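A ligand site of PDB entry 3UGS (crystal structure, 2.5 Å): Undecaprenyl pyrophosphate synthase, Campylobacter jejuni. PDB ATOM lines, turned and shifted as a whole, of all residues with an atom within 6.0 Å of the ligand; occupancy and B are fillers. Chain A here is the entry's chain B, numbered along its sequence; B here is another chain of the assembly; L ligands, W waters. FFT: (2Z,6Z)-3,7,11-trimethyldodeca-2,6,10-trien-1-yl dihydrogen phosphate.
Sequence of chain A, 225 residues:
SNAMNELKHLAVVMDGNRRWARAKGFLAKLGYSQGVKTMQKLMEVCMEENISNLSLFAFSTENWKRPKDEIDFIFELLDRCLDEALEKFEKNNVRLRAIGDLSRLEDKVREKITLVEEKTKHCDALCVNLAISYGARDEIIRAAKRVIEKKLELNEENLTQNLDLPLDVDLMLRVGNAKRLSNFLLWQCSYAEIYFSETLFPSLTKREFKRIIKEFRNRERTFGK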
ATOM      1  N   VAL A  13      25.470 -11.827   0.882  1.00  0.00           N
ATOM      2  CA  VAL A  13      24.357 -10.946   1.136  1.00  0.00           C
ATOM      3  C   VAL A  13      23.098 -11.757   1.344  1.00  0.00           C
ATOM      4  O   VAL A  13      22.800 -12.721   0.647  1.00  0.00           O
ATOM      5  CB  VAL A  13      24.099  -9.908   0.037  1.00  0.00           C
ATOM      6  CG1 VAL A  13      23.850 -10.582  -1.298  1.00  0.00           C
ATOM      7  CG2 VAL A  13      22.890  -9.018   0.442  1.00  0.00           C
ATOM      8  N   MET A  14      22.336 -11.342   2.342  1.00  0.00           N
ATOM      9  CA  MET A  14      21.054 -12.021   2.659  1.00  0.00           C
ATOM     10  C   MET A  14      19.892 -11.121   2.296  1.00  0.00           C
ATOM     11  O   MET A  14      20.017  -9.916   2.250  1.00  0.00           O
ATOM     12  CB  MET A  14      21.001 -12.397   4.129  1.00  0.00           C
ATOM     13  CG  MET A  14      22.283 -13.087   4.588  1.00  0.00           C
ATOM     14  SD  MET A  14      22.694 -12.676   6.296  1.00  0.00           S
ATOM     15  CE  MET A  14      24.280 -13.508   6.465  1.00  0.00           C
ATOM     16  N   ASP A  15      18.766 -11.726   2.023  1.00  0.00           N
ATOM     17  CA  ASP A  15      17.546 -10.957   1.764  1.00  0.00           C
ATOM     18  C   ASP A  15      17.391  -9.873   2.826  1.00  0.00           C
ATOM     19  O   ASP A  15      17.449 -10.096   4.010  1.00  0.00           O
ATOM     20  CB  ASP A  15      16.306 -11.813   1.770  1.00  0.00           C
ATOM     21  CG  ASP A  15      16.080 -12.513   0.462  1.00  0.00           C
ATOM     22  OD1 ASP A  15      14.964 -13.046   0.305  1.00  0.00           O
ATOM     23  OD2 ASP A  15      17.008 -12.538  -0.403  1.00  0.00           O
ATOM     24  N   GLY A  16      17.207  -8.679   2.336  1.00  0.00           N
ATOM     25  CA  GLY A  16      16.995  -7.536   3.195  1.00  0.00           C
ATOM     26  C   GLY A  16      15.533  -7.138   3.381  1.00  0.00           C
ATOM     27  O   GLY A  16      15.264  -6.068   3.946  1.00  0.00           O
ATOM     28  N   ASN A  17      14.598  -7.951   2.913  1.00  0.00           N
ATOM     29  CA  ASN A  17      13.158  -7.606   3.170  1.00  0.00           C
ATOM     30  C   ASN A  17      12.415  -8.402   4.256  1.00  0.00           C
ATOM     31  O   ASN A  17      13.025  -9.075   5.066  1.00  0.00           O
ATOM     32  CB  ASN A  17      12.321  -7.509   1.891  1.00  0.00           C
ATOM     33  CG  ASN A  17      12.210  -8.829   1.145  1.00  0.00           C
ATOM     34  OD1 ASN A  17      12.108  -9.895   1.759  1.00  0.00           O
ATOM     35  ND2 ASN A  17      12.198  -8.751  -0.186  1.00  0.00           N
ATOM     36  N   PHE A  57      27.310  -7.860   3.953  1.00  0.00           N
ATOM     37  CA  PHE A  57      26.550  -6.670   3.641  1.00  0.00           C
ATOM     38  C   PHE A  57      25.584  -6.337   4.757  1.00  0.00           C
ATOM     39  O   PHE A  57      24.585  -6.972   4.918  1.00  0.00           O
ATOM     40  CB  PHE A  57      25.756  -6.799   2.320  1.00  0.00           C
ATOM     41  CG  PHE A  57      25.528  -5.482   1.599  1.00  0.00           C
ATOM     42  CD1 PHE A  57      25.841  -4.268   2.197  1.00  0.00           C
ATOM     43  CD2 PHE A  57      25.023  -5.462   0.322  1.00  0.00           C
ATOM     44  CE1 PHE A  57      25.657  -3.074   1.506  1.00  0.00           C
ATOM     45  CE2 PHE A  57      24.845  -4.279  -0.363  1.00  0.00           C
ATOM     46  CZ  PHE A  57      25.150  -3.095   0.225  1.00  0.00           C
ATOM     47  N   ALA A  58      25.896  -5.278   5.474  1.00  0.00           N
ATOM     48  CA  ALA A  58      25.061  -4.876   6.628  1.00  0.00           C
ATOM     49  C   ALA A  58      24.030  -3.810   6.282  1.00  0.00           C
ATOM     50  O   ALA A  58      22.838  -3.990   6.507  1.00  0.00           O
ATOM     51  CB  ALA A  58      25.947  -4.399   7.767  1.00  0.00           C
ATOM     52  N   PHE A  59      24.531  -2.708   5.745  1.00  0.00           N
ATOM     53  CA  PHE A  59      23.738  -1.501   5.459  1.00  0.00           C
ATOM     54  C   PHE A  59      24.332  -0.746   4.235  1.00  0.00           C
ATOM     55  O   PHE A  59      25.551  -0.488   4.123  1.00  0.00           O
ATOM     56  CB  PHE A  59      23.695  -0.552   6.679  1.00  0.00           C
ATOM     57  CG  PHE A  59      22.639   0.540   6.593  1.00  0.00           C
ATOM     58  CD1 PHE A  59      21.369   0.340   7.069  1.00  0.00           C
ATOM     59  CD2 PHE A  59      22.946   1.786   6.056  1.00  0.00           C
ATOM     60  CE1 PHE A  59      20.402   1.359   7.025  1.00  0.00           C
ATOM     61  CE2 PHE A  59      21.999   2.804   5.980  1.00  0.00           C
ATOM     62  CZ  PHE A  59      20.720   2.592   6.444  1.00  0.00           C
ATOM     63  N   SER A  60      23.441  -0.357   3.354  1.00  0.00           N
ATOM     64  CA  SER A  60      23.876   0.295   2.134  1.00  0.00           C
ATOM     65  C   SER A  60      23.529   1.753   2.075  1.00  0.00           C
ATOM     66  O   SER A  60      22.816   2.255   2.923  1.00  0.00           O
ATOM     67  CB  SER A  60      23.266  -0.389   0.915  1.00  0.00           C
ATOM     68  OG  SER A  60      21.860  -0.203   0.898  1.00  0.00           O
ATOM     69  N   ASN A  63      19.776   2.157   1.637  1.00  0.00           N
ATOM     70  CA  ASN A  63      19.091   1.780   2.893  1.00  0.00           C
ATOM     71  C   ASN A  63      18.729   3.006   3.749  1.00  0.00           C
ATOM     72  O   ASN A  63      17.849   2.954   4.626  1.00  0.00           O
ATOM     73  CB  ASN A  63      19.907   0.805   3.748  1.00  0.00           C
ATOM     74  CG  ASN A  63      19.942  -0.617   3.179  1.00  0.00           C
ATOM     75  OD1 ASN A  63      20.853  -1.397   3.496  1.00  0.00           O
ATOM     76  ND2 ASN A  63      18.993  -0.953   2.357  1.00  0.00           N
ATOM     77  N   ARG A  66      15.143   3.955   3.829  1.00  0.00           N
ATOM     78  CA  ARG A  66      14.261   3.100   4.653  1.00  0.00           C
ATOM     79  C   ARG A  66      13.604   3.905   5.766  1.00  0.00           C
ATOM     80  O   ARG A  66      14.189   4.848   6.289  1.00  0.00           O
ATOM     81  CB  ARG A  66      15.049   1.998   5.349  1.00  0.00           C
ATOM     82  CG  ARG A  66      15.261   0.712   4.542  1.00  0.00           C
ATOM     83  CD  ARG A  66      16.032  -0.215   5.466  1.00  0.00           C
ATOM     84  NE  ARG A  66      16.495  -1.439   4.844  1.00  0.00           N
ATOM     85  CZ  ARG A  66      15.825  -2.572   4.829  1.00  0.00           C
ATOM     86  NH1 ARG A  66      14.634  -2.663   5.392  1.00  0.00           N
ATOM     87  NH2 ARG A  66      16.368  -3.638   4.241  1.00  0.00           N
ATOM     88  N   ILE A  74      18.150  -2.118  12.801  1.00  0.00           N
ATOM     89  CA  ILE A  74      19.357  -2.624  12.133  1.00  0.00           C
ATOM     90  C   ILE A  74      20.649  -2.192  12.829  1.00  0.00           C
ATOM     91  O   ILE A  74      21.537  -2.986  13.028  1.00  0.00           O
ATOM     92  CB  ILE A  74      19.394  -2.179  10.668  1.00  0.00           C
ATOM     93  CG1 ILE A  74      18.302  -2.903   9.909  1.00  0.00           C
ATOM     94  CG2 ILE A  74      20.746  -2.495  10.013  1.00  0.00           C
ATOM     95  CD1 ILE A  74      17.935  -2.209   8.614  1.00  0.00           C
ATOM     96  N   PHE A  75      20.705  -0.927  13.192  1.00  0.00           N
ATOM     97  CA  PHE A  75      21.871  -0.345  13.927  1.00  0.00           C
ATOM     98  C   PHE A  75      21.895  -0.852  15.343  1.00  0.00           C
ATOM     99  O   PHE A  75      22.928  -0.968  15.968  1.00  0.00           O
ATOM    100  CB  PHE A  75      21.900   1.197  13.895  1.00  0.00           C
ATOM    101  CG  PHE A  75      22.410   1.721  12.586  1.00  0.00           C
ATOM    102  CD1 PHE A  75      23.683   1.394  12.124  1.00  0.00           C
ATOM    103  CD2 PHE A  75      21.592   2.443  11.756  1.00  0.00           C
ATOM    104  CE1 PHE A  75      24.129   1.803  10.890  1.00  0.00           C
ATOM    105  CE2 PHE A  75      22.049   2.852  10.513  1.00  0.00           C
ATOM    106  CZ  PHE A  75      23.304   2.531  10.075  1.00  0.00           C
ATOM    107  N   LEU A  77      20.971  -3.931  16.228  1.00  0.00           N
ATOM    108  CA  LEU A  77      21.628  -5.267  16.042  1.00  0.00           C
ATOM    109  C   LEU A  77      23.103  -5.181  15.692  1.00  0.00           C
ATOM    110  O   LEU A  77      23.959  -5.895  16.199  1.00  0.00           O
ATOM    111  CB  LEU A  77      20.958  -6.070  14.949  1.00  0.00           C
ATOM    112  CG  LEU A  77      19.462  -6.259  15.159  1.00  0.00           C
ATOM    113  CD1 LEU A  77      18.832  -6.730  13.842  1.00  0.00           C
ATOM    114  CD2 LEU A  77      19.109  -7.205  16.328  1.00  0.00           C
ATOM    115  N   LEU A  78      23.371  -4.315  14.742  1.00  0.00           N
ATOM    116  CA  LEU A  78      24.760  -4.100  14.289  1.00  0.00           C
ATOM    117  C   LEU A  78      25.644  -3.832  15.521  1.00  0.00           C
ATOM    118  O   LEU A  78      26.746  -4.359  15.697  1.00  0.00           O
ATOM    119  CB  LEU A  78      24.849  -2.929  13.304  1.00  0.00           C
ATOM    120  CG  LEU A  78      26.293  -2.452  13.126  1.00  0.00           C
ATOM    121  CD1 LEU A  78      27.090  -3.468  12.314  1.00  0.00           C
ATOM    122  CD2 LEU A  78      26.344  -1.066  12.491  1.00  0.00           C
ATOM    123  N   CYS A  81      26.230  -6.911  17.326  1.00  0.00           N
ATOM    124  CA  CYS A  81      27.264  -7.676  16.574  1.00  0.00           C
ATOM    125  C   CYS A  81      28.657  -7.105  16.771  1.00  0.00           C
ATOM    126  O   CYS A  81      29.658  -7.816  16.774  1.00  0.00           O
ATOM    127  CB  CYS A  81      26.981  -7.735  15.087  1.00  0.00           C
ATOM    128  SG  CYS A  81      25.440  -8.582  14.704  1.00  0.00           S
ATOM    129  N   ARG A 174      24.254 -15.235  -2.521  1.00  0.00           N
ATOM    130  CA  ARG A 174      22.996 -14.640  -2.059  1.00  0.00           C
ATOM    131  C   ARG A 174      22.242 -15.689  -1.227  1.00  0.00           C
ATOM    132  O   ARG A 174      21.980 -16.794  -1.683  1.00  0.00           O
ATOM    133  CB  ARG A 174      22.132 -14.138  -3.218  1.00  0.00           C
ATOM    134  CG  ARG A 174      20.654 -14.000  -2.890  1.00  0.00           C
ATOM    135  CD  ARG A 174      20.319 -12.820  -1.956  1.00  0.00           C
ATOM    136  NE  ARG A 174      20.569 -11.514  -2.595  1.00  0.00           N
ATOM    137  CZ  ARG A 174      20.041 -10.349  -2.210  1.00  0.00           C
ATOM    138  NH1 ARG A 174      19.249 -10.275  -1.155  1.00  0.00           N
ATOM    139  NH2 ARG A 174      20.318  -9.240  -2.877  1.00  0.00           N
ATOM    140  N   ALA A 178      15.720 -13.098  -3.108  1.00  0.00           N
ATOM    141  CA  ALA A 178      16.087 -11.956  -3.999  1.00  0.00           C
ATOM    142  C   ALA A 178      17.177 -12.360  -4.986  1.00  0.00           C
ATOM    143  O   ALA A 178      18.150 -12.995  -4.625  1.00  0.00           O
ATOM    144  CB  ALA A 178      16.568 -10.737  -3.206  1.00  0.00           C
ATOM    145  N   ARG A 180      19.635 -10.624  -7.251  1.00  0.00           N
ATOM    146  CA  ARG A 180      20.228  -9.310  -7.537  1.00  0.00           C
ATOM    147  C   ARG A 180      21.388  -8.996  -6.625  1.00  0.00           C
ATOM    148  O   ARG A 180      21.560  -9.662  -5.624  1.00  0.00           O
ATOM    149  CB  ARG A 180      19.178  -8.224  -7.436  1.00  0.00           C
ATOM    150  CG  ARG A 180      18.514  -8.193  -6.069  1.00  0.00           C
ATOM    151  CD  ARG A 180      17.472  -7.108  -5.991  1.00  0.00           C
ATOM    152  NE  ARG A 180      16.776  -7.113  -4.709  1.00  0.00           N
ATOM    153  CZ  ARG A 180      15.449  -7.173  -4.556  1.00  0.00           C
ATOM    154  NH1 ARG A 180      14.645  -7.253  -5.620  1.00  0.00           N
ATOM    155  NH2 ARG A 180      14.938  -7.118  -3.337  1.00  0.00           N
ATOM    156  N   LEU A 181      22.213  -8.027  -7.026  1.00  0.00           N
ATOM    157  CA  LEU A 181      23.445  -7.687  -6.249  1.00  0.00           C
ATOM    158  C   LEU A 181      23.280  -6.519  -5.319  1.00  0.00           C
ATOM    159  O   LEU A 181      24.043  -6.307  -4.416  1.00  0.00           O
ATOM    160  CB  LEU A 181      24.646  -7.442  -7.155  1.00  0.00           C
ATOM    161  CG  LEU A 181      25.094  -8.689  -7.973  1.00  0.00           C
ATOM    162  CD1 LEU A 181      26.489  -8.446  -8.530  1.00  0.00           C
ATOM    163  CD2 LEU A 181      25.089  -9.963  -7.146  1.00  0.00           C
ATOM    164  N   SER A 182      22.244  -5.774  -5.599  1.00  0.00           N
ATOM    165  CA  SER A 182      21.874  -4.604  -4.809  1.00  0.00           C
ATOM    166  C   SER A 182      23.066  -3.754  -4.384  1.00  0.00           C
ATOM    167  O   SER A 182      23.353  -3.592  -3.214  1.00  0.00           O
ATOM    168  CB  SER A 182      21.097  -5.029  -3.579  1.00  0.00           C
ATOM    169  OG  SER A 182      19.846  -5.505  -3.991  1.00  0.00           O
ATOM    170  N   TYR B 191      21.021  -2.479  -9.341  1.00  0.00           N
ATOM    171  CA  TYR B 191      19.707  -3.042  -8.905  1.00  0.00           C
ATOM    172  C   TYR B 191      18.984  -3.930  -9.898  1.00  0.00           C
ATOM    173  O   TYR B 191      17.823  -4.238  -9.726  1.00  0.00           O
ATOM    174  CB  TYR B 191      18.769  -1.971  -8.376  1.00  0.00           C
ATOM    175  CG  TYR B 191      19.221  -1.548  -6.999  1.00  0.00           C
ATOM    176  CD1 TYR B 191      18.889  -2.299  -5.889  1.00  0.00           C
ATOM    177  CD2 TYR B 191      20.066  -0.464  -6.836  1.00  0.00           C
ATOM    178  CE1 TYR B 191      19.370  -1.975  -4.646  1.00  0.00           C
ATOM    179  CE2 TYR B 191      20.531  -0.111  -5.578  1.00  0.00           C
ATOM    180  CZ  TYR B 191      20.202  -0.892  -4.488  1.00  0.00           C
ATOM    181  OH  TYR B 191      20.649  -0.511  -3.229  1.00  0.00           O
ATOM    182  N   THR B 222      12.717  -3.280  -4.422  1.00  0.00           N
ATOM    183  CA  THR B 222      12.754  -2.204  -3.404  1.00  0.00           C
ATOM    184  C   THR B 222      13.760  -1.100  -3.691  1.00  0.00           C
ATOM    185  O   THR B 222      13.748  -0.050  -3.058  1.00  0.00           O
ATOM    186  CB  THR B 222      13.037  -2.765  -2.018  1.00  0.00           C
ATOM    187  OG1 THR B 222      14.276  -3.451  -2.047  1.00  0.00           O
ATOM    188  CG2 THR B 222      11.914  -3.745  -1.569  1.00  0.00           C
ATOM    189  N   GLY B 224      16.543  -0.819  -2.650  1.00  0.00           N
ATOM    190  CA  GLY B 224      17.092  -0.576  -1.290  1.00  0.00           C
ATOM    191  C   GLY B 224      16.189   0.142  -0.290  1.00  0.00           C
ATOM    192  O   GLY B 224      16.629   0.405   0.834  1.00  0.00           O
HETATM  193  O3  FFT L   1      18.537  -7.133  -2.442  1.00  0.00           O
HETATM  194  P   FFT L   1      17.898  -6.928  -1.097  1.00  0.00           P
HETATM  195  O1  FFT L   1      17.788  -8.192  -0.296  1.00  0.00           O
HETATM  196  O2  FFT L   1      16.643  -6.071  -1.206  1.00  0.00           O
HETATM  197  O   FFT L   1      18.893  -6.028  -0.184  1.00  0.00           O
HETATM  198  C14 FFT L   1      20.120  -6.568   0.323  1.00  0.00           C
HETATM  199  C13 FFT L   1      20.972  -5.485   0.952  1.00  0.00           C
HETATM  200  C11 FFT L   1      21.405  -5.540   2.207  1.00  0.00           C
HETATM  201  C12 FFT L   1      22.233  -4.445   2.774  1.00  0.00           C
HETATM  202  C10 FFT L   1      21.159  -6.751   3.076  1.00  0.00           C
HETATM  203  C9  FFT L   1      20.484  -6.401   4.359  1.00  0.00           C
HETATM  204  C8  FFT L   1      19.981  -7.663   5.036  1.00  0.00           C
HETATM  205  C6  FFT L   1      20.487  -8.095   6.205  1.00  0.00           C
HETATM  206  C7  FFT L   1      19.964  -9.335   6.891  1.00  0.00           C
HETATM  207  C5  FFT L   1      21.588  -7.302   6.864  1.00  0.00           C
HETATM  208  C4  FFT L   1      21.413  -7.498   8.356  1.00  0.00           C
HETATM  209  C3  FFT L   1      22.222  -6.495   9.155  1.00  0.00           C
HETATM  210  C1  FFT L   1      22.463  -6.751  10.461  1.00  0.00           C
HETATM  211  C2  FFT L   1      21.945  -8.015  11.120  1.00  0.00           C
HETATM  212  C   FFT L   1      23.275  -5.742  11.252  1.00  0.00           C
HETATM  213  O   HOH W   1      15.304  -9.468  -0.434  1.00  0.00           O
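Merely in contact with the ligand: Asn 63, Asp 15, Met 14, Ala 58, Phe 57, Thr 222 of chain B, Val 13, Ile 74 and Leu 78.
Hydrophobic or aromatic side chains that line the ligand: Val 13, Phe 57 and Leu 78.
The nearest printed residue that does not touch the ligand is Ala 178 (4.1 Å).
O3 of the ligand lies within hydrogen-bond range of OG of Ser 182.
NH1 of Arg 174 lies within salt-bridge range of O1 of the ligand (2.7 Å).
N of Gly 16 lies within hydrogen-bond range of O1 of the ligand (2.7 Å).
NE of Arg 180 lies within salt-bridge range of O3 of the ligand, 2.9 Å away.
Water W1 lies within hydrogen-bond range of an oxygen (O1) of the ligand (2.8 Å), the side-chain amide nitrogen (ND2) of Asn 17 (3.2 Å) and the backbone NH (N) of Gly 16 (3.5 Å).
O of Arg 180 is in hydrogen-bond range of NH2 of Arg 174 (3.0 Å).
OD2 of Asp 15 is in salt-bridge range of NH1 of Arg 174.
NE of Arg 174 sits close to O of Ala 178 (3.5 Å).
O of Gly 16 sits at hydrogen-bond distance from NH2 of Arg 66 (2.7 Å).
The backbone NH of Ser 60 is in hydrogen-bond range of the side-chain amide oxygen of Asn 63, 2.8 Å away.
The side-chain amide nitrogen (ND2) of Asn 63 lies within hydrogen-bond range of the backbone carbonyl oxygen (O) of Gly 224 of chain B (3.1 Å).
The side-chain carboxylate of Asp 15 sits at hydrogen-bond distance from the backbone NH of Ala 178, 3.0 Å away.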
